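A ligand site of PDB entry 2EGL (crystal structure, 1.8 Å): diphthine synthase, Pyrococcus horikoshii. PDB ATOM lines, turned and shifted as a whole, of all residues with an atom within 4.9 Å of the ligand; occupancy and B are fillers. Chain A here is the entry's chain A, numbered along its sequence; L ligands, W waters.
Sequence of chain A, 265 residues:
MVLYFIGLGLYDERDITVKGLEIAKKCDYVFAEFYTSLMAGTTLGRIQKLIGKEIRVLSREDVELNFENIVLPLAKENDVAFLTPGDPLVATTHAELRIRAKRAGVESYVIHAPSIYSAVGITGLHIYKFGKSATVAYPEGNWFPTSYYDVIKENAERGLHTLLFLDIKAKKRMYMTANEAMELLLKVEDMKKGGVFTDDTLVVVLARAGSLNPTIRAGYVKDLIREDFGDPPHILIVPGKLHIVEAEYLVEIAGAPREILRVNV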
ATOM      1  N   LEU A  10     -30.408 -21.251  -5.959  1.00  0.00           N
ATOM      2  CA  LEU A  10     -30.109 -21.136  -4.532  1.00  0.00           C
ATOM      3  C   LEU A  10     -31.136 -21.249  -3.423  1.00  0.00           C
ATOM      4  O   LEU A  10     -30.884 -21.909  -2.416  1.00  0.00           O
ATOM      5  CB  LEU A  10     -29.391 -19.806  -4.297  1.00  0.00           C
ATOM      6  CG  LEU A  10     -28.129 -19.518  -5.119  1.00  0.00           C
ATOM      7  CD1 LEU A  10     -27.843 -18.026  -5.104  1.00  0.00           C
ATOM      8  CD2 LEU A  10     -26.964 -20.307  -4.582  1.00  0.00           C
ATOM      9  N   TYR A  11     -32.287 -20.601  -3.589  1.00  0.00           N
ATOM     10  CA  TYR A  11     -33.258 -20.540  -2.503  1.00  0.00           C
ATOM     11  C   TYR A  11     -34.702 -20.919  -2.785  1.00  0.00           C
ATOM     12  O   TYR A  11     -35.280 -21.727  -2.051  1.00  0.00           O
ATOM     13  CB  TYR A  11     -33.190 -19.106  -1.954  1.00  0.00           C
ATOM     14  CG  TYR A  11     -34.021 -18.841  -0.722  1.00  0.00           C
ATOM     15  CD1 TYR A  11     -33.673 -19.405   0.500  1.00  0.00           C
ATOM     16  CD2 TYR A  11     -35.133 -17.999  -0.778  1.00  0.00           C
ATOM     17  CE1 TYR A  11     -34.416 -19.137   1.656  1.00  0.00           C
ATOM     18  CE2 TYR A  11     -35.882 -17.729   0.362  1.00  0.00           C
ATOM     19  CZ  TYR A  11     -35.523 -18.299   1.573  1.00  0.00           C
ATOM     20  OH  TYR A  11     -36.260 -18.041   2.695  1.00  0.00           O
ATOM     21  N   THR A  36     -28.755 -33.172  -2.626  1.00  0.00           N
ATOM     22  CA  THR A  36     -27.433 -32.539  -2.738  1.00  0.00           C
ATOM     23  C   THR A  36     -27.371 -31.173  -2.051  1.00  0.00           C
ATOM     24  O   THR A  36     -26.294 -30.710  -1.679  1.00  0.00           O
ATOM     25  CB  THR A  36     -26.997 -32.364  -4.208  1.00  0.00           C
ATOM     26  OG1 THR A  36     -27.988 -31.630  -4.932  1.00  0.00           O
ATOM     27  CG2 THR A  36     -26.789 -33.713  -4.858  1.00  0.00           C
ATOM     28  N   SER A  37     -28.522 -30.527  -1.895  1.00  0.00           N
ATOM     29  CA  SER A  37     -28.579 -29.225  -1.256  1.00  0.00           C
ATOM     30  C   SER A  37     -29.979 -28.927  -0.749  1.00  0.00           C
ATOM     31  O   SER A  37     -30.914 -29.685  -1.015  1.00  0.00           O
ATOM     32  CB  SER A  37     -28.140 -28.137  -2.245  1.00  0.00           C
ATOM     33  OG  SER A  37     -27.967 -26.901  -1.575  1.00  0.00           O
ATOM     34  N   LEU A  38     -30.118 -27.826  -0.024  1.00  0.00           N
ATOM     35  CA  LEU A  38     -31.407 -27.430   0.526  1.00  0.00           C
ATOM     36  C   LEU A  38     -31.908 -26.099  -0.028  1.00  0.00           C
ATOM     37  O   LEU A  38     -31.218 -25.088   0.057  1.00  0.00           O
ATOM     38  CB  LEU A  38     -31.324 -27.332   2.044  1.00  0.00           C
ATOM     39  CG  LEU A  38     -32.595 -26.824   2.752  1.00  0.00           C
ATOM     40  CD1 LEU A  38     -33.711 -27.858   2.595  1.00  0.00           C
ATOM     41  CD2 LEU A  38     -32.315 -26.572   4.224  1.00  0.00           C
ATOM     42  N   PRO A  85     -30.955 -28.732  -7.078  1.00  0.00           N
ATOM     43  CA  PRO A  85     -30.814 -27.418  -6.432  1.00  0.00           C
ATOM     44  C   PRO A  85     -29.544 -26.777  -6.988  1.00  0.00           C
ATOM     45  O   PRO A  85     -28.668 -27.488  -7.505  1.00  0.00           O
ATOM     46  CB  PRO A  85     -30.642 -27.782  -4.946  1.00  0.00           C
ATOM     47  CG  PRO A  85     -31.353 -29.108  -4.837  1.00  0.00           C
ATOM     48  CD  PRO A  85     -30.923 -29.817  -6.091  1.00  0.00           C
ATOM     49  N   GLY A  86     -29.432 -25.459  -6.875  1.00  0.00           N
ATOM     50  CA  GLY A  86     -28.261 -24.742  -7.368  1.00  0.00           C
ATOM     51  C   GLY A  86     -27.920 -25.095  -8.803  1.00  0.00           C
ATOM     52  O   GLY A  86     -28.814 -25.176  -9.646  1.00  0.00           O
ATOM     53  N   ASP A  87     -26.635 -25.289  -9.078  1.00  0.00           N
ATOM     54  CA  ASP A  87     -26.168 -25.669 -10.408  1.00  0.00           C
ATOM     55  C   ASP A  87     -25.998 -27.193 -10.336  1.00  0.00           C
ATOM     56  O   ASP A  87     -25.339 -27.710  -9.437  1.00  0.00           O
ATOM     57  CB  ASP A  87     -24.846 -24.976 -10.724  1.00  0.00           C
ATOM     58  CG  ASP A  87     -24.325 -25.309 -12.113  1.00  0.00           C
ATOM     59  OD1 ASP A  87     -23.960 -26.480 -12.348  1.00  0.00           O
ATOM     60  OD2 ASP A  87     -24.278 -24.398 -12.973  1.00  0.00           O
ATOM     61  N   VAL A  90     -22.242 -28.613  -9.806  1.00  0.00           N
ATOM     62  CA  VAL A  90     -21.365 -28.016  -8.802  1.00  0.00           C
ATOM     63  C   VAL A  90     -21.459 -28.725  -7.467  1.00  0.00           C
ATOM     64  O   VAL A  90     -22.540 -28.786  -6.865  1.00  0.00           O
ATOM     65  CB  VAL A  90     -21.688 -26.522  -8.590  1.00  0.00           C
ATOM     66  CG1 VAL A  90     -20.884 -25.989  -7.399  1.00  0.00           C
ATOM     67  CG2 VAL A  90     -21.358 -25.728  -9.839  1.00  0.00           C
ATOM     68  N   ALA A  91     -20.342 -29.250  -6.980  1.00  0.00           N
ATOM     69  CA  ALA A  91     -20.306 -29.934  -5.691  1.00  0.00           C
ATOM     70  C   ALA A  91     -21.271 -31.104  -5.651  1.00  0.00           C
ATOM     71  O   ALA A  91     -21.842 -31.428  -4.603  1.00  0.00           O
ATOM     72  CB  ALA A  91     -20.625 -28.947  -4.570  1.00  0.00           C
ATOM     73  N   THR A  92     -21.463 -31.735  -6.808  1.00  0.00           N
ATOM     74  CA  THR A  92     -22.231 -32.946  -6.945  1.00  0.00           C
ATOM     75  C   THR A  92     -21.406 -33.915  -7.771  1.00  0.00           C
ATOM     76  O   THR A  92     -20.358 -33.584  -8.311  1.00  0.00           O
ATOM     77  CB  THR A  92     -23.565 -32.653  -7.657  1.00  0.00           C
ATOM     78  OG1 THR A  92     -23.329 -32.471  -9.064  1.00  0.00           O
ATOM     79  CG2 THR A  92     -24.224 -31.386  -7.100  1.00  0.00           C
ATOM     80  N   PRO A 114     -27.942 -20.193 -10.529  1.00  0.00           N
ATOM     81  CA  PRO A 114     -27.079 -19.612  -9.491  1.00  0.00           C
ATOM     82  C   PRO A 114     -26.553 -20.704  -8.559  1.00  0.00           C
ATOM     83  O   PRO A 114     -27.314 -21.570  -8.115  1.00  0.00           O
ATOM     84  CB  PRO A 114     -28.021 -18.665  -8.747  1.00  0.00           C
ATOM     85  CG  PRO A 114     -29.047 -18.299  -9.777  1.00  0.00           C
ATOM     86  CD  PRO A 114     -29.283 -19.583 -10.522  1.00  0.00           C
ATOM     87  N   SER A 115     -25.259 -20.646  -8.257  1.00  0.00           N
ATOM     88  CA  SER A 115     -24.624 -21.629  -7.387  1.00  0.00           C
ATOM     89  C   SER A 115     -24.012 -20.943  -6.177  1.00  0.00           C
ATOM     90  O   SER A 115     -23.587 -19.791  -6.264  1.00  0.00           O
ATOM     91  CB  SER A 115     -23.514 -22.345  -8.171  1.00  0.00           C
ATOM     92  OG  SER A 115     -22.753 -23.179  -7.334  1.00  0.00           O
ATOM     93  N   ILE A 116     -23.961 -21.646  -5.050  1.00  0.00           N
ATOM     94  CA  ILE A 116     -23.383 -21.061  -3.843  1.00  0.00           C
ATOM     95  C   ILE A 116     -21.901 -20.775  -4.066  1.00  0.00           C
ATOM     96  O   ILE A 116     -21.342 -19.862  -3.459  1.00  0.00           O
ATOM     97  CB  ILE A 116     -23.549 -22.005  -2.627  1.00  0.00           C
ATOM     98  CG1 ILE A 116     -23.106 -21.286  -1.357  1.00  0.00           C
ATOM     99  CG2 ILE A 116     -22.758 -23.291  -2.845  1.00  0.00           C
ATOM    100  CD1 ILE A 116     -23.963 -20.062  -1.015  1.00  0.00           C
ATOM    101  N   TYR A 117     -21.280 -21.539  -4.964  1.00  0.00           N
ATOM    102  CA  TYR A 117     -19.867 -21.389  -5.267  1.00  0.00           C
ATOM    103  C   TYR A 117     -19.540 -19.969  -5.738  1.00  0.00           C
ATOM    104  O   TYR A 117     -18.484 -19.426  -5.425  1.00  0.00           O
ATOM    105  CB  TYR A 117     -19.456 -22.429  -6.310  1.00  0.00           C
ATOM    106  CG  TYR A 117     -17.982 -22.462  -6.672  1.00  0.00           C
ATOM    107  CD1 TYR A 117     -17.011 -22.765  -5.720  1.00  0.00           C
ATOM    108  CD2 TYR A 117     -17.568 -22.227  -7.979  1.00  0.00           C
ATOM    109  CE1 TYR A 117     -15.653 -22.831  -6.060  1.00  0.00           C
ATOM    110  CE2 TYR A 117     -16.225 -22.288  -8.338  1.00  0.00           C
ATOM    111  CZ  TYR A 117     -15.268 -22.594  -7.382  1.00  0.00           C
ATOM    112  OH  TYR A 117     -13.942 -22.649  -7.745  1.00  0.00           O
ATOM    113  N   PHE A 165     -18.200 -25.963   2.323  1.00  0.00           N
ATOM    114  CA  PHE A 165     -19.553 -26.455   2.126  1.00  0.00           C
ATOM    115  C   PHE A 165     -19.837 -27.203   3.423  1.00  0.00           C
ATOM    116  O   PHE A 165     -18.940 -27.834   3.982  1.00  0.00           O
ATOM    117  CB  PHE A 165     -19.594 -27.449   0.952  1.00  0.00           C
ATOM    118  CG  PHE A 165     -19.291 -26.830  -0.383  1.00  0.00           C
ATOM    119  CD1 PHE A 165     -20.297 -26.220  -1.132  1.00  0.00           C
ATOM    120  CD2 PHE A 165     -17.995 -26.873  -0.908  1.00  0.00           C
ATOM    121  CE1 PHE A 165     -20.017 -25.664  -2.378  1.00  0.00           C
ATOM    122  CE2 PHE A 165     -17.715 -26.317  -2.154  1.00  0.00           C
ATOM    123  CZ  PHE A 165     -18.725 -25.713  -2.895  1.00  0.00           C
ATOM    124  N   LEU A 166     -21.077 -27.143   3.923  1.00  0.00           N
ATOM    125  CA  LEU A 166     -21.400 -27.835   5.160  1.00  0.00           C
ATOM    126  C   LEU A 166     -22.214 -29.095   4.887  1.00  0.00           C
ATOM    127  O   LEU A 166     -22.992 -29.146   3.935  1.00  0.00           O
ATOM    128  CB  LEU A 166     -22.146 -26.882   6.116  1.00  0.00           C
ATOM    129  CG  LEU A 166     -21.402 -25.566   6.395  1.00  0.00           C
ATOM    130  CD1 LEU A 166     -22.110 -24.794   7.505  1.00  0.00           C
ATOM    131  CD2 LEU A 166     -19.963 -25.857   6.802  1.00  0.00           C
ATOM    132  N   ASP A 167     -22.041 -30.108   5.729  1.00  0.00           N
ATOM    133  CA  ASP A 167     -22.717 -31.384   5.534  1.00  0.00           C
ATOM    134  C   ASP A 167     -24.250 -31.337   5.523  1.00  0.00           C
ATOM    135  O   ASP A 167     -24.876 -30.429   6.058  1.00  0.00           O
ATOM    136  CB  ASP A 167     -22.259 -32.395   6.579  1.00  0.00           C
ATOM    137  CG  ASP A 167     -22.321 -33.828   6.090  1.00  0.00           C
ATOM    138  OD1 ASP A 167     -22.840 -34.055   4.969  1.00  0.00           O
ATOM    139  OD2 ASP A 167     -21.850 -34.735   6.819  1.00  0.00           O
ATOM    140  N   ILE A 168     -24.836 -32.348   4.891  1.00  0.00           N
ATOM    141  CA  ILE A 168     -26.273 -32.466   4.798  1.00  0.00           C
ATOM    142  C   ILE A 168     -26.679 -33.937   4.805  1.00  0.00           C
ATOM    143  O   ILE A 168     -26.018 -34.771   4.195  1.00  0.00           O
ATOM    144  CB  ILE A 168     -26.805 -31.801   3.500  1.00  0.00           C
ATOM    145  CG1 ILE A 168     -28.315 -32.022   3.381  1.00  0.00           C
ATOM    146  CG2 ILE A 168     -26.078 -32.366   2.303  1.00  0.00           C
ATOM    147  CD1 ILE A 168     -28.946 -31.293   2.206  1.00  0.00           C
ATOM    148  N   LEU A 206     -22.512 -17.176   5.595  1.00  0.00           N
ATOM    149  CA  LEU A 206     -23.527 -16.768   4.620  1.00  0.00           C
ATOM    150  C   LEU A 206     -24.638 -17.792   4.740  1.00  0.00           C
ATOM    151  O   LEU A 206     -24.438 -18.965   4.469  1.00  0.00           O
ATOM    152  CB  LEU A 206     -22.955 -16.789   3.204  1.00  0.00           C
ATOM    153  CG  LEU A 206     -23.975 -16.542   2.080  1.00  0.00           C
ATOM    154  CD1 LEU A 206     -24.673 -15.194   2.276  1.00  0.00           C
ATOM    155  CD2 LEU A 206     -23.244 -16.581   0.740  1.00  0.00           C
ATOM    156  N   ALA A 207     -25.813 -17.330   5.154  1.00  0.00           N
ATOM    157  CA  ALA A 207     -26.956 -18.221   5.324  1.00  0.00           C
ATOM    158  C   ALA A 207     -28.102 -17.839   4.396  1.00  0.00           C
ATOM    159  O   ALA A 207     -28.458 -16.671   4.267  1.00  0.00           O
ATOM    160  CB  ALA A 207     -27.434 -18.187   6.774  1.00  0.00           C
ATOM    161  N   ARG A 208     -28.664 -18.858   3.742  1.00  0.00           N
ATOM    162  CA  ARG A 208     -29.787 -18.679   2.829  1.00  0.00           C
ATOM    163  C   ARG A 208     -29.493 -17.733   1.671  1.00  0.00           C
ATOM    164  O   ARG A 208     -30.279 -16.839   1.361  1.00  0.00           O
ATOM    165  CB  ARG A 208     -31.019 -18.219   3.618  1.00  0.00           C
ATOM    166  CG  ARG A 208     -31.422 -19.203   4.727  1.00  0.00           C
ATOM    167  CD  ARG A 208     -32.592 -18.667   5.542  1.00  0.00           C
ATOM    168  NE  ARG A 208     -32.328 -17.308   5.998  1.00  0.00           N
ATOM    169  CZ  ARG A 208     -31.441 -16.980   6.942  1.00  0.00           C
ATOM    170  NH1 ARG A 208     -30.732 -17.925   7.547  1.00  0.00           N
ATOM    171  NH2 ARG A 208     -31.248 -15.713   7.255  1.00  0.00           N
ATOM    172  N   ALA A 209     -28.342 -17.932   1.037  1.00  0.00           N
ATOM    173  CA  ALA A 209     -27.985 -17.114  -0.121  1.00  0.00           C
ATOM    174  C   ALA A 209     -29.118 -17.348  -1.124  1.00  0.00           C
ATOM    175  O   ALA A 209     -29.694 -18.436  -1.166  1.00  0.00           O
ATOM    176  CB  ALA A 209     -26.670 -17.588  -0.706  1.00  0.00           C
ATOM    177  N   GLY A 210     -29.435 -16.334  -1.919  1.00  0.00           N
ATOM    178  CA  GLY A 210     -30.508 -16.490  -2.882  1.00  0.00           C
ATOM    179  C   GLY A 210     -31.759 -15.780  -2.391  1.00  0.00           C
ATOM    180  O   GLY A 210     -32.542 -15.252  -3.181  1.00  0.00           O
ATOM    181  N   PRO A 233     -29.934 -23.391   4.575  1.00  0.00           N
ATOM    182  CA  PRO A 233     -28.553 -23.849   4.617  1.00  0.00           C
ATOM    183  C   PRO A 233     -27.555 -22.749   4.973  1.00  0.00           C
ATOM    184  O   PRO A 233     -27.838 -21.564   4.800  1.00  0.00           O
ATOM    185  CB  PRO A 233     -28.330 -24.391   3.214  1.00  0.00           C
ATOM    186  CG  PRO A 233     -29.124 -23.454   2.386  1.00  0.00           C
ATOM    187  CD  PRO A 233     -30.405 -23.286   3.177  1.00  0.00           C
ATOM    188  N   HIS A 234     -26.402 -23.159   5.475  1.00  0.00           N
ATOM    189  CA  HIS A 234     -25.334 -22.242   5.862  1.00  0.00           C
ATOM    190  C   HIS A 234     -24.066 -22.666   5.150  1.00  0.00           C
ATOM    191  O   HIS A 234     -23.911 -23.827   4.779  1.00  0.00           O
ATOM    192  CB  HIS A 234     -25.015 -22.334   7.355  1.00  0.00           C
ATOM    193  CG  HIS A 234     -26.105 -21.868   8.270  1.00  0.00           C
ATOM    194  ND1 HIS A 234     -25.958 -21.859   9.638  1.00  0.00           N
ATOM    195  CD2 HIS A 234     -27.345 -21.387   8.017  1.00  0.00           C
ATOM    196  CE1 HIS A 234     -27.061 -21.395  10.193  1.00  0.00           C
ATOM    197  NE2 HIS A 234     -27.925 -21.108   9.231  1.00  0.00           N
ATOM    198  N   ILE A 235     -23.159 -21.728   4.987  1.00  0.00           N
ATOM    199  CA  ILE A 235     -21.864 -22.028   4.420  1.00  0.00           C
ATOM    200  C   ILE A 235     -20.901 -21.204   5.276  1.00  0.00           C
ATOM    201  O   ILE A 235     -21.264 -20.123   5.748  1.00  0.00           O
ATOM    202  CB  ILE A 235     -21.786 -21.650   2.916  1.00  0.00           C
ATOM    203  CG1 ILE A 235     -20.709 -22.500   2.243  1.00  0.00           C
ATOM    204  CG2 ILE A 235     -21.473 -20.168   2.741  1.00  0.00           C
ATOM    205  CD1 ILE A 235     -21.051 -22.893   0.818  1.00  0.00           C
HETATM  206  N1  LIG L   1     -24.892 -27.772  -6.597  1.00  0.00           N
HETATM  207  C1  LIG L   1     -25.128 -26.901  -5.369  1.00  0.00           C
HETATM  208  C2  LIG L   1     -24.292 -27.168  -4.153  1.00  0.00           C
HETATM  209  C3  LIG L   1     -24.312 -28.557  -3.528  1.00  0.00           C
HETATM  210  S1  LIG L   1     -23.330 -28.427  -1.977  1.00  0.00           S
HETATM  211  C4  LIG L   1     -24.928 -25.397  -5.828  1.00  0.00           C
HETATM  212  O1  LIG L   1     -24.615 -25.166  -7.012  1.00  0.00           O
HETATM  213  O2  LIG L   1     -25.117 -24.488  -4.923  1.00  0.00           O
HETATM  214  C5  LIG L   1     -24.613 -28.115  -0.831  1.00  0.00           C
HETATM  215  C6  LIG L   1     -24.052 -27.224   0.349  1.00  0.00           C
HETATM  216  O3  LIG L   1     -23.726 -25.927  -0.195  1.00  0.00           O
HETATM  217  C7  LIG L   1     -24.999 -27.005   1.465  1.00  0.00           C
HETATM  218  O4  LIG L   1     -24.919 -28.048   2.413  1.00  0.00           O
HETATM  219  C8  LIG L   1     -24.553 -25.610   1.980  1.00  0.00           C
HETATM  220  O5  LIG L   1     -23.451 -25.700   2.885  1.00  0.00           O
HETATM  221  C9  LIG L   1     -24.227 -24.824   0.696  1.00  0.00           C
HETATM  222  N2  LIG L   1     -25.273 -24.185   0.131  1.00  0.00           N
HETATM  223  C10 LIG L   1     -26.111 -24.437  -0.934  1.00  0.00           C
HETATM  224  N3  LIG L   1     -27.022 -23.547  -1.148  1.00  0.00           N
HETATM  225  C11 LIG L   1     -26.803 -22.570  -0.129  1.00  0.00           C
HETATM  226  C12 LIG L   1     -27.489 -21.334   0.163  1.00  0.00           C
HETATM  227  N4  LIG L   1     -28.534 -20.858  -0.534  1.00  0.00           N
HETATM  228  N5  LIG L   1     -26.980 -20.639   1.239  1.00  0.00           N
HETATM  229  C13 LIG L   1     -25.921 -21.073   1.978  1.00  0.00           C
HETATM  230  N6  LIG L   1     -25.247 -22.250   1.727  1.00  0.00           N
HETATM  231  C14 LIG L   1     -25.747 -22.941   0.661  1.00  0.00           C
HETATM  232  O   HOH W   1     -26.267 -28.212   4.807  1.00  0.00           O
HETATM  233  O   HOH W   2     -27.090 -29.312  -5.828  1.00  0.00           O
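N1 of the ligand lies within hydrogen-bond range of O of Val 90, at 2.6 Å.
N of Leu 166 is in hydrogen-bond range of O5 of the ligand.
O of Leu 166 sits at hydrogen-bond distance from O4 of the ligand (2.7 Å).
The backbone carbonyl oxygen of His 234 sits at hydrogen-bond distance from an oxygen (O5) of the ligand, 2.7 Å away.
An oxygen (O1) of the ligand lies within hydrogen-bond range of the side-chain hydroxyl (OG) of Ser 115 (2.7 Å).
N5 of the ligand sits at hydrogen-bond distance from N of Ala 209 (3.0 Å).
The backbone carbonyl oxygen of Ala 209 sits at hydrogen-bond distance from a nitrogen (N4) of the ligand (2.8 Å).
The backbone NH (N) of Asp 87 sits at hydrogen-bond distance from an oxygen (O1) of the ligand (2.9 Å).
N1 of the ligand is in hydrogen-bond range of O of Asp 87, 2.9 Å away.
The backbone NH of Ile 116 sits at hydrogen-bond distance from an oxygen (O2) of the ligand (3.1 Å).
The backbone carbonyl oxygen of Leu 10 sits at hydrogen-bond distance from a nitrogen (N4) of the ligand (3.2 Å).
The backbone carbonyl oxygen (O) of Thr 36 sits close to a sulfur (S1) of the ligand, 3.8 Å away.
Ser 37 touches the ligand (OG to C10, 3.2 Å).
Pro 85 touches the ligand (O to N1, 3.9 Å).
Gly 86 touches the ligand (CA to O1, 3.7 Å).
CB of Ala 91 touches S1 of the ligand (3.8 Å).
Thr 92 touches the ligand.
Phe 165 touches the ligand.
Leu 206 touches the ligand (O to C13, 3.6 Å).
Arg 208 touches the ligand.
Pro 233 touches the ligand.
Ile 235 touches the ligand.
Of the 27 residues printed, 19 come within 4 Å of the ligand.
The nearest printed residue that does not touch the ligand is Ile 168 (4.3 Å).
The backbone NH (N) of Tyr 117 sits close to the side-chain hydroxyl (OG) of Ser 115, 3.2 Å away.
The backbone carbonyl oxygen (O) of Pro 233 lies within hydrogen-bond range of the backbone NH (N) of Arg 208, at 3.0 Å.
N of Ile 235 lies within hydrogen-bond range of O of Leu 206, 3.1 Å away.
Water W1 lies within hydrogen-bond range of O4 of the ligand and O of Asp 167.
Water W2 lies within hydrogen-bond range of the side-chain hydroxyl of Thr 36 (2.6 Å), a nitrogen (N1) of the ligand (2.8 Å) and the backbone carbonyl oxygen of Pro 85 (2.9 Å).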
